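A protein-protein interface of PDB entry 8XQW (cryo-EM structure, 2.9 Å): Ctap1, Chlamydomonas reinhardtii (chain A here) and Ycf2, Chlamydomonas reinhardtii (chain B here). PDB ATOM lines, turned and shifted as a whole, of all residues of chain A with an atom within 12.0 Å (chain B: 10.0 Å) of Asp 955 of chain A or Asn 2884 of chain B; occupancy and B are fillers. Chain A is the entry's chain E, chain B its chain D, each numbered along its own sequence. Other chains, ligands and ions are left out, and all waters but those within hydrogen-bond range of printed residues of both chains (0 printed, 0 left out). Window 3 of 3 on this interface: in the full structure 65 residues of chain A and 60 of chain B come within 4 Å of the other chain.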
ATOM      1  N   VAL A 858       3.109 -22.131  23.676  1.00  0.00           N
ATOM      2  CA  VAL A 858       4.048 -21.480  22.780  1.00  0.00           C
ATOM      3  C   VAL A 858       3.314 -20.570  21.814  1.00  0.00           C
ATOM      4  O   VAL A 858       3.893 -19.636  21.266  1.00  0.00           O
ATOM      5  CB  VAL A 858       4.886 -22.529  22.030  1.00  0.00           C
ATOM      6  CG1 VAL A 858       5.965 -21.861  21.241  1.00  0.00           C
ATOM      7  CG2 VAL A 858       5.478 -23.496  23.004  1.00  0.00           C
ATOM      8  N   TRP A 946      11.325 -19.092  15.182  1.00  0.00           N
ATOM      9  CA  TRP A 946      11.016 -20.264  16.008  1.00  0.00           C
ATOM     10  C   TRP A 946      11.369 -20.137  17.479  1.00  0.00           C
ATOM     11  O   TRP A 946      10.482 -20.364  18.307  1.00  0.00           O
ATOM     12  CB  TRP A 946      11.694 -21.535  15.486  1.00  0.00           C
ATOM     13  CG  TRP A 946      11.851 -22.591  16.555  1.00  0.00           C
ATOM     14  CD1 TRP A 946      13.012 -23.140  16.985  1.00  0.00           C
ATOM     15  CD2 TRP A 946      10.811 -23.224  17.310  1.00  0.00           C
ATOM     16  NE1 TRP A 946      12.770 -24.064  17.959  1.00  0.00           N
ATOM     17  CE2 TRP A 946      11.422 -24.136  18.175  1.00  0.00           C
ATOM     18  CE3 TRP A 946       9.426 -23.102  17.342  1.00  0.00           C
ATOM     19  CZ2 TRP A 946      10.704 -24.919  19.058  1.00  0.00           C
ATOM     20  CZ3 TRP A 946       8.715 -23.885  18.219  1.00  0.00           C
ATOM     21  CH2 TRP A 946       9.353 -24.779  19.061  1.00  0.00           C
ATOM     22  N   PRO A 947      12.596 -19.818  17.885  1.00  0.00           N
ATOM     23  CA  PRO A 947      12.844 -19.761  19.329  1.00  0.00           C
ATOM     24  C   PRO A 947      12.032 -18.684  20.013  1.00  0.00           C
ATOM     25  O   PRO A 947      11.744 -18.812  21.204  1.00  0.00           O
ATOM     26  CB  PRO A 947      14.349 -19.496  19.425  1.00  0.00           C
ATOM     27  CG  PRO A 947      14.883 -19.792  18.091  1.00  0.00           C
ATOM     28  CD  PRO A 947      13.802 -19.471  17.125  1.00  0.00           C
ATOM     29  N   TYR A 948      11.618 -17.646  19.287  1.00  0.00           N
ATOM     30  CA  TYR A 948      10.873 -16.526  19.856  1.00  0.00           C
ATOM     31  C   TYR A 948      11.587 -15.940  21.060  1.00  0.00           C
ATOM     32  O   TYR A 948      10.953 -15.496  22.013  1.00  0.00           O
ATOM     33  CB  TYR A 948       9.444 -16.923  20.230  1.00  0.00           C
ATOM     34  CG  TYR A 948       8.681 -17.579  19.114  1.00  0.00           C
ATOM     35  CD1 TYR A 948       8.511 -16.945  17.906  1.00  0.00           C
ATOM     36  CD2 TYR A 948       8.132 -18.831  19.269  1.00  0.00           C
ATOM     37  CE1 TYR A 948       7.830 -17.543  16.887  1.00  0.00           C
ATOM     38  CE2 TYR A 948       7.451 -19.433  18.252  1.00  0.00           C
ATOM     39  CZ  TYR A 948       7.301 -18.784  17.064  1.00  0.00           C
ATOM     40  OH  TYR A 948       6.614 -19.380  16.040  1.00  0.00           O
ATOM     41  N   GLY A 949      12.912 -15.944  21.030  1.00  0.00           N
ATOM     42  CA  GLY A 949      13.672 -15.374  22.116  1.00  0.00           C
ATOM     43  C   GLY A 949      13.635 -16.150  23.406  1.00  0.00           C
ATOM     44  O   GLY A 949      14.027 -15.610  24.440  1.00  0.00           O
ATOM     45  N   ILE A 950      13.166 -17.392  23.390  1.00  0.00           N
ATOM     46  CA  ILE A 950      13.214 -18.253  24.562  1.00  0.00           C
ATOM     47  C   ILE A 950      14.507 -19.046  24.488  1.00  0.00           C
ATOM     48  O   ILE A 950      14.761 -19.745  23.509  1.00  0.00           O
ATOM     49  CB  ILE A 950      12.008 -19.184  24.636  1.00  0.00           C
ATOM     50  CG1 ILE A 950      10.725 -18.390  24.678  1.00  0.00           C
ATOM     51  CG2 ILE A 950      12.081 -19.985  25.877  1.00  0.00           C
ATOM     52  CD1 ILE A 950       9.524 -19.257  24.713  1.00  0.00           C
ATOM     53  N   GLU A 951      15.328 -18.941  25.524  1.00  0.00           N
ATOM     54  CA  GLU A 951      16.623 -19.602  25.489  1.00  0.00           C
ATOM     55  C   GLU A 951      16.492 -21.109  25.647  1.00  0.00           C
ATOM     56  O   GLU A 951      17.260 -21.864  25.045  1.00  0.00           O
ATOM     57  CB  GLU A 951      17.520 -19.026  26.579  1.00  0.00           C
ATOM     58  CG  GLU A 951      18.738 -19.855  26.890  1.00  0.00           C
ATOM     59  CD  GLU A 951      19.784 -19.073  27.653  1.00  0.00           C
ATOM     60  OE1 GLU A 951      20.856 -18.792  27.076  1.00  0.00           O
ATOM     61  OE2 GLU A 951      19.536 -18.735  28.829  1.00  0.00           O
ATOM     62  N   TRP A 952      15.518 -21.563  26.421  1.00  0.00           N
ATOM     63  CA  TRP A 952      15.403 -22.965  26.769  1.00  0.00           C
ATOM     64  C   TRP A 952      14.430 -23.734  25.900  1.00  0.00           C
ATOM     65  O   TRP A 952      14.122 -24.878  26.222  1.00  0.00           O
ATOM     66  CB  TRP A 952      14.976 -23.102  28.222  1.00  0.00           C
ATOM     67  CG  TRP A 952      13.766 -22.326  28.554  1.00  0.00           C
ATOM     68  CD1 TRP A 952      13.721 -21.085  29.084  1.00  0.00           C
ATOM     69  CD2 TRP A 952      12.415 -22.744  28.393  1.00  0.00           C
ATOM     70  NE1 TRP A 952      12.425 -20.696  29.266  1.00  0.00           N
ATOM     71  CE2 TRP A 952      11.603 -21.704  28.846  1.00  0.00           C
ATOM     72  CE3 TRP A 952      11.813 -23.901  27.909  1.00  0.00           C
ATOM     73  CZ2 TRP A 952      10.228 -21.780  28.820  1.00  0.00           C
ATOM     74  CZ3 TRP A 952      10.449 -23.972  27.888  1.00  0.00           C
ATOM     75  CH2 TRP A 952       9.671 -22.922  28.338  1.00  0.00           C
ATOM     76  N   LEU A 953      13.926 -23.145  24.821  1.00  0.00           N
ATOM     77  CA  LEU A 953      12.874 -23.813  24.070  1.00  0.00           C
ATOM     78  C   LEU A 953      13.393 -25.030  23.336  1.00  0.00           C
ATOM     79  O   LEU A 953      12.644 -25.981  23.112  1.00  0.00           O
ATOM     80  CB  LEU A 953      12.235 -22.855  23.082  1.00  0.00           C
ATOM     81  CG  LEU A 953      10.836 -23.277  22.693  1.00  0.00           C
ATOM     82  CD1 LEU A 953       9.989 -23.322  23.915  1.00  0.00           C
ATOM     83  CD2 LEU A 953      10.268 -22.315  21.713  1.00  0.00           C
ATOM     84  N   ASP A 954      14.658 -25.024  22.947  1.00  0.00           N
ATOM     85  CA  ASP A 954      15.194 -26.144  22.198  1.00  0.00           C
ATOM     86  C   ASP A 954      15.656 -27.286  23.084  1.00  0.00           C
ATOM     87  O   ASP A 954      16.036 -28.334  22.562  1.00  0.00           O
ATOM     88  CB  ASP A 954      16.339 -25.662  21.325  1.00  0.00           C
ATOM     89  CG  ASP A 954      15.865 -24.785  20.199  1.00  0.00           C
ATOM     90  OD1 ASP A 954      14.955 -25.216  19.463  1.00  0.00           O
ATOM     91  OD2 ASP A 954      16.389 -23.664  20.053  1.00  0.00           O
ATOM     92  N   ASP A 955      15.641 -27.110  24.398  1.00  0.00           N
ATOM     93  CA  ASP A 955      15.891 -28.203  25.321  1.00  0.00           C
ATOM     94  C   ASP A 955      14.613 -28.829  25.838  1.00  0.00           C
ATOM     95  O   ASP A 955      14.685 -29.774  26.622  1.00  0.00           O
ATOM     96  CB  ASP A 955      16.711 -27.730  26.517  1.00  0.00           C
ATOM     97  CG  ASP A 955      18.076 -27.241  26.130  1.00  0.00           C
ATOM     98  OD1 ASP A 955      18.665 -27.805  25.195  1.00  0.00           O
ATOM     99  OD2 ASP A 955      18.572 -26.292  26.768  1.00  0.00           O
ATOM    100  N   ALA A 956      13.460 -28.319  25.444  1.00  0.00           N
ATOM    101  CA  ALA A 956      12.191 -28.823  25.928  1.00  0.00           C
ATOM    102  C   ALA A 956      11.281 -29.339  24.837  1.00  0.00           C
ATOM    103  O   ALA A 956      10.542 -30.287  25.081  1.00  0.00           O
ATOM    104  CB  ALA A 956      11.444 -27.735  26.697  1.00  0.00           C
ATOM    105  N   TYR A 957      11.317 -28.751  23.649  1.00  0.00           N
ATOM    106  CA  TYR A 957      10.410 -29.091  22.575  1.00  0.00           C
ATOM    107  C   TYR A 957      11.187 -29.611  21.380  1.00  0.00           C
ATOM    108  O   TYR A 957      12.199 -29.008  21.002  1.00  0.00           O
ATOM    109  CB  TYR A 957       9.599 -27.876  22.153  1.00  0.00           C
ATOM    110  CG  TYR A 957       8.455 -27.566  23.059  1.00  0.00           C
ATOM    111  CD1 TYR A 957       8.668 -27.021  24.300  1.00  0.00           C
ATOM    112  CD2 TYR A 957       7.168 -27.821  22.677  1.00  0.00           C
ATOM    113  CE1 TYR A 957       7.632 -26.743  25.132  1.00  0.00           C
ATOM    114  CE2 TYR A 957       6.128 -27.542  23.502  1.00  0.00           C
ATOM    115  CZ  TYR A 957       6.363 -27.004  24.727  1.00  0.00           C
ATOM    116  OH  TYR A 957       5.312 -26.726  25.554  1.00  0.00           O
ATOM    117  N   PRO A 958      10.765 -30.704  20.759  1.00  0.00           N
ATOM    118  CA  PRO A 958      11.279 -31.019  19.432  1.00  0.00           C
ATOM    119  C   PRO A 958      10.832 -29.951  18.465  1.00  0.00           C
ATOM    120  O   PRO A 958       9.821 -29.284  18.675  1.00  0.00           O
ATOM    121  CB  PRO A 958      10.634 -32.366  19.110  1.00  0.00           C
ATOM    122  CG  PRO A 958      10.187 -32.891  20.402  1.00  0.00           C
ATOM    123  CD  PRO A 958       9.810 -31.716  21.213  1.00  0.00           C
ATOM    124  N   LYS A 959      11.576 -29.786  17.410  1.00  0.00           N
ATOM    125  CA  LYS A 959      11.217 -28.731  16.482  1.00  0.00           C
ATOM    126  C   LYS A 959      10.005 -29.155  15.664  1.00  0.00           C
ATOM    127  O   LYS A 959       9.992 -30.258  15.119  1.00  0.00           O
ATOM    128  CB  LYS A 959      12.372 -28.406  15.565  1.00  0.00           C
ATOM    129  CG  LYS A 959      12.105 -27.195  14.746  1.00  0.00           C
ATOM    130  CD  LYS A 959      13.322 -26.766  13.988  1.00  0.00           C
ATOM    131  CE  LYS A 959      14.441 -26.436  14.921  1.00  0.00           C
ATOM    132  NZ  LYS A 959      15.506 -25.720  14.188  1.00  0.00           N
ATOM    133  N   PRO A 960       8.973 -28.324  15.575  1.00  0.00           N
ATOM    134  CA  PRO A 960       7.783 -28.690  14.809  1.00  0.00           C
ATOM    135  C   PRO A 960       8.094 -28.887  13.337  1.00  0.00           C
ATOM    136  O   PRO A 960       9.230 -28.773  12.885  1.00  0.00           O
ATOM    137  CB  PRO A 960       6.861 -27.495  15.020  1.00  0.00           C
ATOM    138  CG  PRO A 960       7.268 -26.949  16.299  1.00  0.00           C
ATOM    139  CD  PRO A 960       8.743 -27.120  16.377  1.00  0.00           C
ATOM    140  N   TRP B2880       6.172 -27.746  30.175  1.00  0.00           N
ATOM    141  CA  TRP B2880       7.404 -28.456  29.867  1.00  0.00           C
ATOM    142  C   TRP B2880       8.587 -27.521  30.013  1.00  0.00           C
ATOM    143  O   TRP B2880       8.537 -26.372  29.585  1.00  0.00           O
ATOM    144  CB  TRP B2880       7.353 -29.009  28.450  1.00  0.00           C
ATOM    145  CG  TRP B2880       6.261 -29.970  28.259  1.00  0.00           C
ATOM    146  CD1 TRP B2880       4.964 -29.690  28.019  1.00  0.00           C
ATOM    147  CD2 TRP B2880       6.363 -31.387  28.315  1.00  0.00           C
ATOM    148  NE1 TRP B2880       4.241 -30.842  27.917  1.00  0.00           N
ATOM    149  CE2 TRP B2880       5.083 -31.901  28.101  1.00  0.00           C
ATOM    150  CE3 TRP B2880       7.415 -32.272  28.530  1.00  0.00           C
ATOM    151  CZ2 TRP B2880       4.826 -33.256  28.087  1.00  0.00           C
ATOM    152  CZ3 TRP B2880       7.157 -33.610  28.516  1.00  0.00           C
ATOM    153  CH2 TRP B2880       5.876 -34.093  28.296  1.00  0.00           C
ATOM    154  N   LEU B2881       9.653 -28.004  30.636  1.00  0.00           N
ATOM    155  CA  LEU B2881      10.790 -27.126  30.850  1.00  0.00           C
ATOM    156  C   LEU B2881      12.108 -27.750  30.433  1.00  0.00           C
ATOM    157  O   LEU B2881      13.008 -27.045  29.985  1.00  0.00           O
ATOM    158  CB  LEU B2881      10.854 -26.708  32.310  1.00  0.00           C
ATOM    159  CG  LEU B2881      11.900 -25.675  32.688  1.00  0.00           C
ATOM    160  CD1 LEU B2881      11.363 -24.297  32.474  1.00  0.00           C
ATOM    161  CD2 LEU B2881      12.268 -25.857  34.125  1.00  0.00           C
ATOM    162  N   LEU B2882      12.240 -29.061  30.566  1.00  0.00           N
ATOM    163  CA  LEU B2882      13.512 -29.690  30.251  1.00  0.00           C
ATOM    164  C   LEU B2882      13.355 -31.186  30.069  1.00  0.00           C
ATOM    165  O   LEU B2882      12.794 -31.857  30.931  1.00  0.00           O
ATOM    166  CB  LEU B2882      14.529 -29.416  31.352  1.00  0.00           C
ATOM    167  CG  LEU B2882      15.814 -30.224  31.264  1.00  0.00           C
ATOM    168  CD1 LEU B2882      16.722 -29.649  30.236  1.00  0.00           C
ATOM    169  CD2 LEU B2882      16.506 -30.238  32.578  1.00  0.00           C
ATOM    170  N   ASN B2883      13.811 -31.717  28.944  1.00  0.00           N
ATOM    171  CA  ASN B2883      13.960 -33.157  28.825  1.00  0.00           C
ATOM    172  C   ASN B2883      15.224 -33.512  28.069  1.00  0.00           C
ATOM    173  O   ASN B2883      15.210 -34.398  27.216  1.00  0.00           O
ATOM    174  CB  ASN B2883      12.744 -33.795  28.173  1.00  0.00           C
ATOM    175  CG  ASN B2883      12.492 -33.293  26.792  1.00  0.00           C
ATOM    176  OD1 ASN B2883      11.533 -32.572  26.557  1.00  0.00           O
ATOM    177  ND2 ASN B2883      13.335 -33.692  25.854  1.00  0.00           N
ATOM    178  N   ASN B2884      16.322 -32.827  28.363  1.00  0.00           N
ATOM    179  CA  ASN B2884      17.563 -33.016  27.628  1.00  0.00           C
ATOM    180  C   ASN B2884      18.581 -33.825  28.422  1.00  0.00           C
ATOM    181  O   ASN B2884      19.339 -34.608  27.847  1.00  0.00           O
ATOM    182  CB  ASN B2884      18.151 -31.664  27.247  1.00  0.00           C
ATOM    183  CG  ASN B2884      19.241 -31.784  26.231  1.00  0.00           C
ATOM    184  OD1 ASN B2884      20.389 -32.038  26.571  1.00  0.00           O
ATOM    185  ND2 ASN B2884      18.893 -31.605  24.969  1.00  0.00           N
ATOM    186  N   GLY B2885      18.624 -33.634  29.728  1.00  0.00           N
ATOM    187  CA  GLY B2885      19.509 -34.419  30.558  1.00  0.00           C
ATOM    188  C   GLY B2885      18.810 -34.867  31.815  1.00  0.00           C
ATOM    189  O   GLY B2885      19.425 -35.412  32.730  1.00  0.00           O
ATOM    190  N   SER B2886      17.513 -34.642  31.857  1.00  0.00           N
ATOM    191  CA  SER B2886      16.670 -34.923  33.007  1.00  0.00           C
ATOM    192  C   SER B2886      15.240 -34.729  32.537  1.00  0.00           C
ATOM    193  O   SER B2886      14.998 -34.521  31.347  1.00  0.00           O
ATOM    194  CB  SER B2886      17.032 -34.024  34.182  1.00  0.00           C
ATOM    195  OG  SER B2886      16.215 -34.301  35.293  1.00  0.00           O
ATOM    196  N   TRP B2887      14.283 -34.810  33.447  1.00  0.00           N
ATOM    197  CA  TRP B2887      12.892 -34.530  33.122  1.00  0.00           C
ATOM    198  C   TRP B2887      12.359 -33.562  34.158  1.00  0.00           C
ATOM    199  O   TRP B2887      12.167 -33.944  35.312  1.00  0.00           O
ATOM    200  CB  TRP B2887      12.050 -35.804  33.098  1.00  0.00           C
ATOM    201  CG  TRP B2887      12.338 -36.726  31.961  1.00  0.00           C
ATOM    202  CD1 TRP B2887      13.262 -37.715  31.932  1.00  0.00           C
ATOM    203  CD2 TRP B2887      11.688 -36.753  30.695  1.00  0.00           C
ATOM    204  NE1 TRP B2887      13.236 -38.351  30.725  1.00  0.00           N
ATOM    205  CE2 TRP B2887      12.275 -37.774  29.945  1.00  0.00           C
ATOM    206  CE3 TRP B2887      10.665 -36.005  30.119  1.00  0.00           C
ATOM    207  CZ2 TRP B2887      11.880 -38.068  28.657  1.00  0.00           C
ATOM    208  CZ3 TRP B2887      10.279 -36.295  28.842  1.00  0.00           C
ATOM    209  CH2 TRP B2887      10.880 -37.317  28.122  1.00  0.00           C
ATOM    210  N   ASN B2888      12.112 -32.321  33.757  1.00  0.00           N
ATOM    211  CA  ASN B2888      11.633 -31.308  34.678  1.00  0.00           C
ATOM    212  C   ASN B2888      10.399 -30.640  34.116  1.00  0.00           C
ATOM    213  O   ASN B2888      10.199 -30.589  32.905  1.00  0.00           O
ATOM    214  CB  ASN B2888      12.675 -30.239  34.934  1.00  0.00           C
ATOM    215  CG  ASN B2888      13.511 -30.533  36.126  1.00  0.00           C
ATOM    216  OD1 ASN B2888      13.538 -29.765  37.079  1.00  0.00           O
ATOM    217  ND2 ASN B2888      14.211 -31.651  36.092  1.00  0.00           N
ATOM    218  N   PHE B2889       9.578 -30.072  34.994  1.00  0.00           N
ATOM    219  CA  PHE B2889       8.365 -29.308  34.602  1.00  0.00           C
ATOM    220  C   PHE B2889       8.450 -27.986  35.344  1.00  0.00           C
ATOM    221  O   PHE B2889       9.312 -27.901  36.199  1.00  0.00           O
ATOM    222  CB  PHE B2889       7.126 -30.144  34.885  1.00  0.00           C
ATOM    223  CG  PHE B2889       6.717 -31.127  33.804  1.00  0.00           C
ATOM    224  CD1 PHE B2889       7.366 -32.344  33.667  1.00  0.00           C
ATOM    225  CD2 PHE B2889       5.655 -30.848  32.960  1.00  0.00           C
ATOM    226  CE1 PHE B2889       6.982 -33.241  32.691  1.00  0.00           C
ATOM    227  CE2 PHE B2889       5.274 -31.753  31.990  1.00  0.00           C
ATOM    228  CZ  PHE B2889       5.936 -32.945  31.862  1.00  0.00           C
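OD1 of Asn 2883 of chain B sits close to O of Ala 956 of chain A (2.9 Å). N of Asn 2883 of chain B sits at hydrogen-bond distance from O of Asp 955 of chain A (3.2 Å).
N of Asn 2888 of chain B is in hydrogen-bond range of O of Leu 2882 of chain B (2.9 Å). O of Asn 2888 of chain B is in hydrogen-bond range of N of Leu 2881 of chain B (3.5 Å).
Among the printed residues, merely in contact across the chains: Trp 952 of chain A with Trp 2880 of chain B, Ala 956 of chain A with Leu 2881 of chain B, Asp 955 of chain A with Asn 2884 of chain B, Asp 955 of chain A with Leu 2882 of chain B, Tyr 957 of chain A with Trp 2880 of chain B and Trp 952 of chain A with Leu 2881 of chain B.
Of chain B, only Leu 2882, Asn 2883 and Asn 2884 come within 4 Å of Asp 955 of chain A. Of chain B, only Leu 2881 (3.7 Å) and Asn 2883 (2.9 Å) come within 4 Å of Ala 956 of chain A. Printed residues of chain A within 4 Å of Leu 2882 of chain B: Asp 955. No residue of chain A comes within 4 Å of Gly 2885 of chain B. Of the printed residues of chain A, Trp 2880 of chain B touches Trp 952 and Tyr 957. Of the printed residues of chain B, Trp 952 of chain A touches Trp 2880 and Leu 2881. Of the printed residues of chain B, Tyr 957 of chain A touches Trp 2880 (3.9 Å). Printed residues of chain A within 4 Å of Leu 2881 of chain B: Trp 952 and Ala 956. Trp 946 of chain A touches none of the printed residues of chain B. The nearest printed residue of chain A that does not touch Leu 2881 of chain B is Asp 955 of chain A (4.6 Å).
Of the 10 printed residues of chain B, 5 touch a printed residue of chain A. Of the 16 printed residues of chain A, 4 touch a printed residue of chain B. Hydrophobic or aromatic side chains of chain A that line the printed part of chain B: Trp 952, Ala 956 and Tyr 957.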
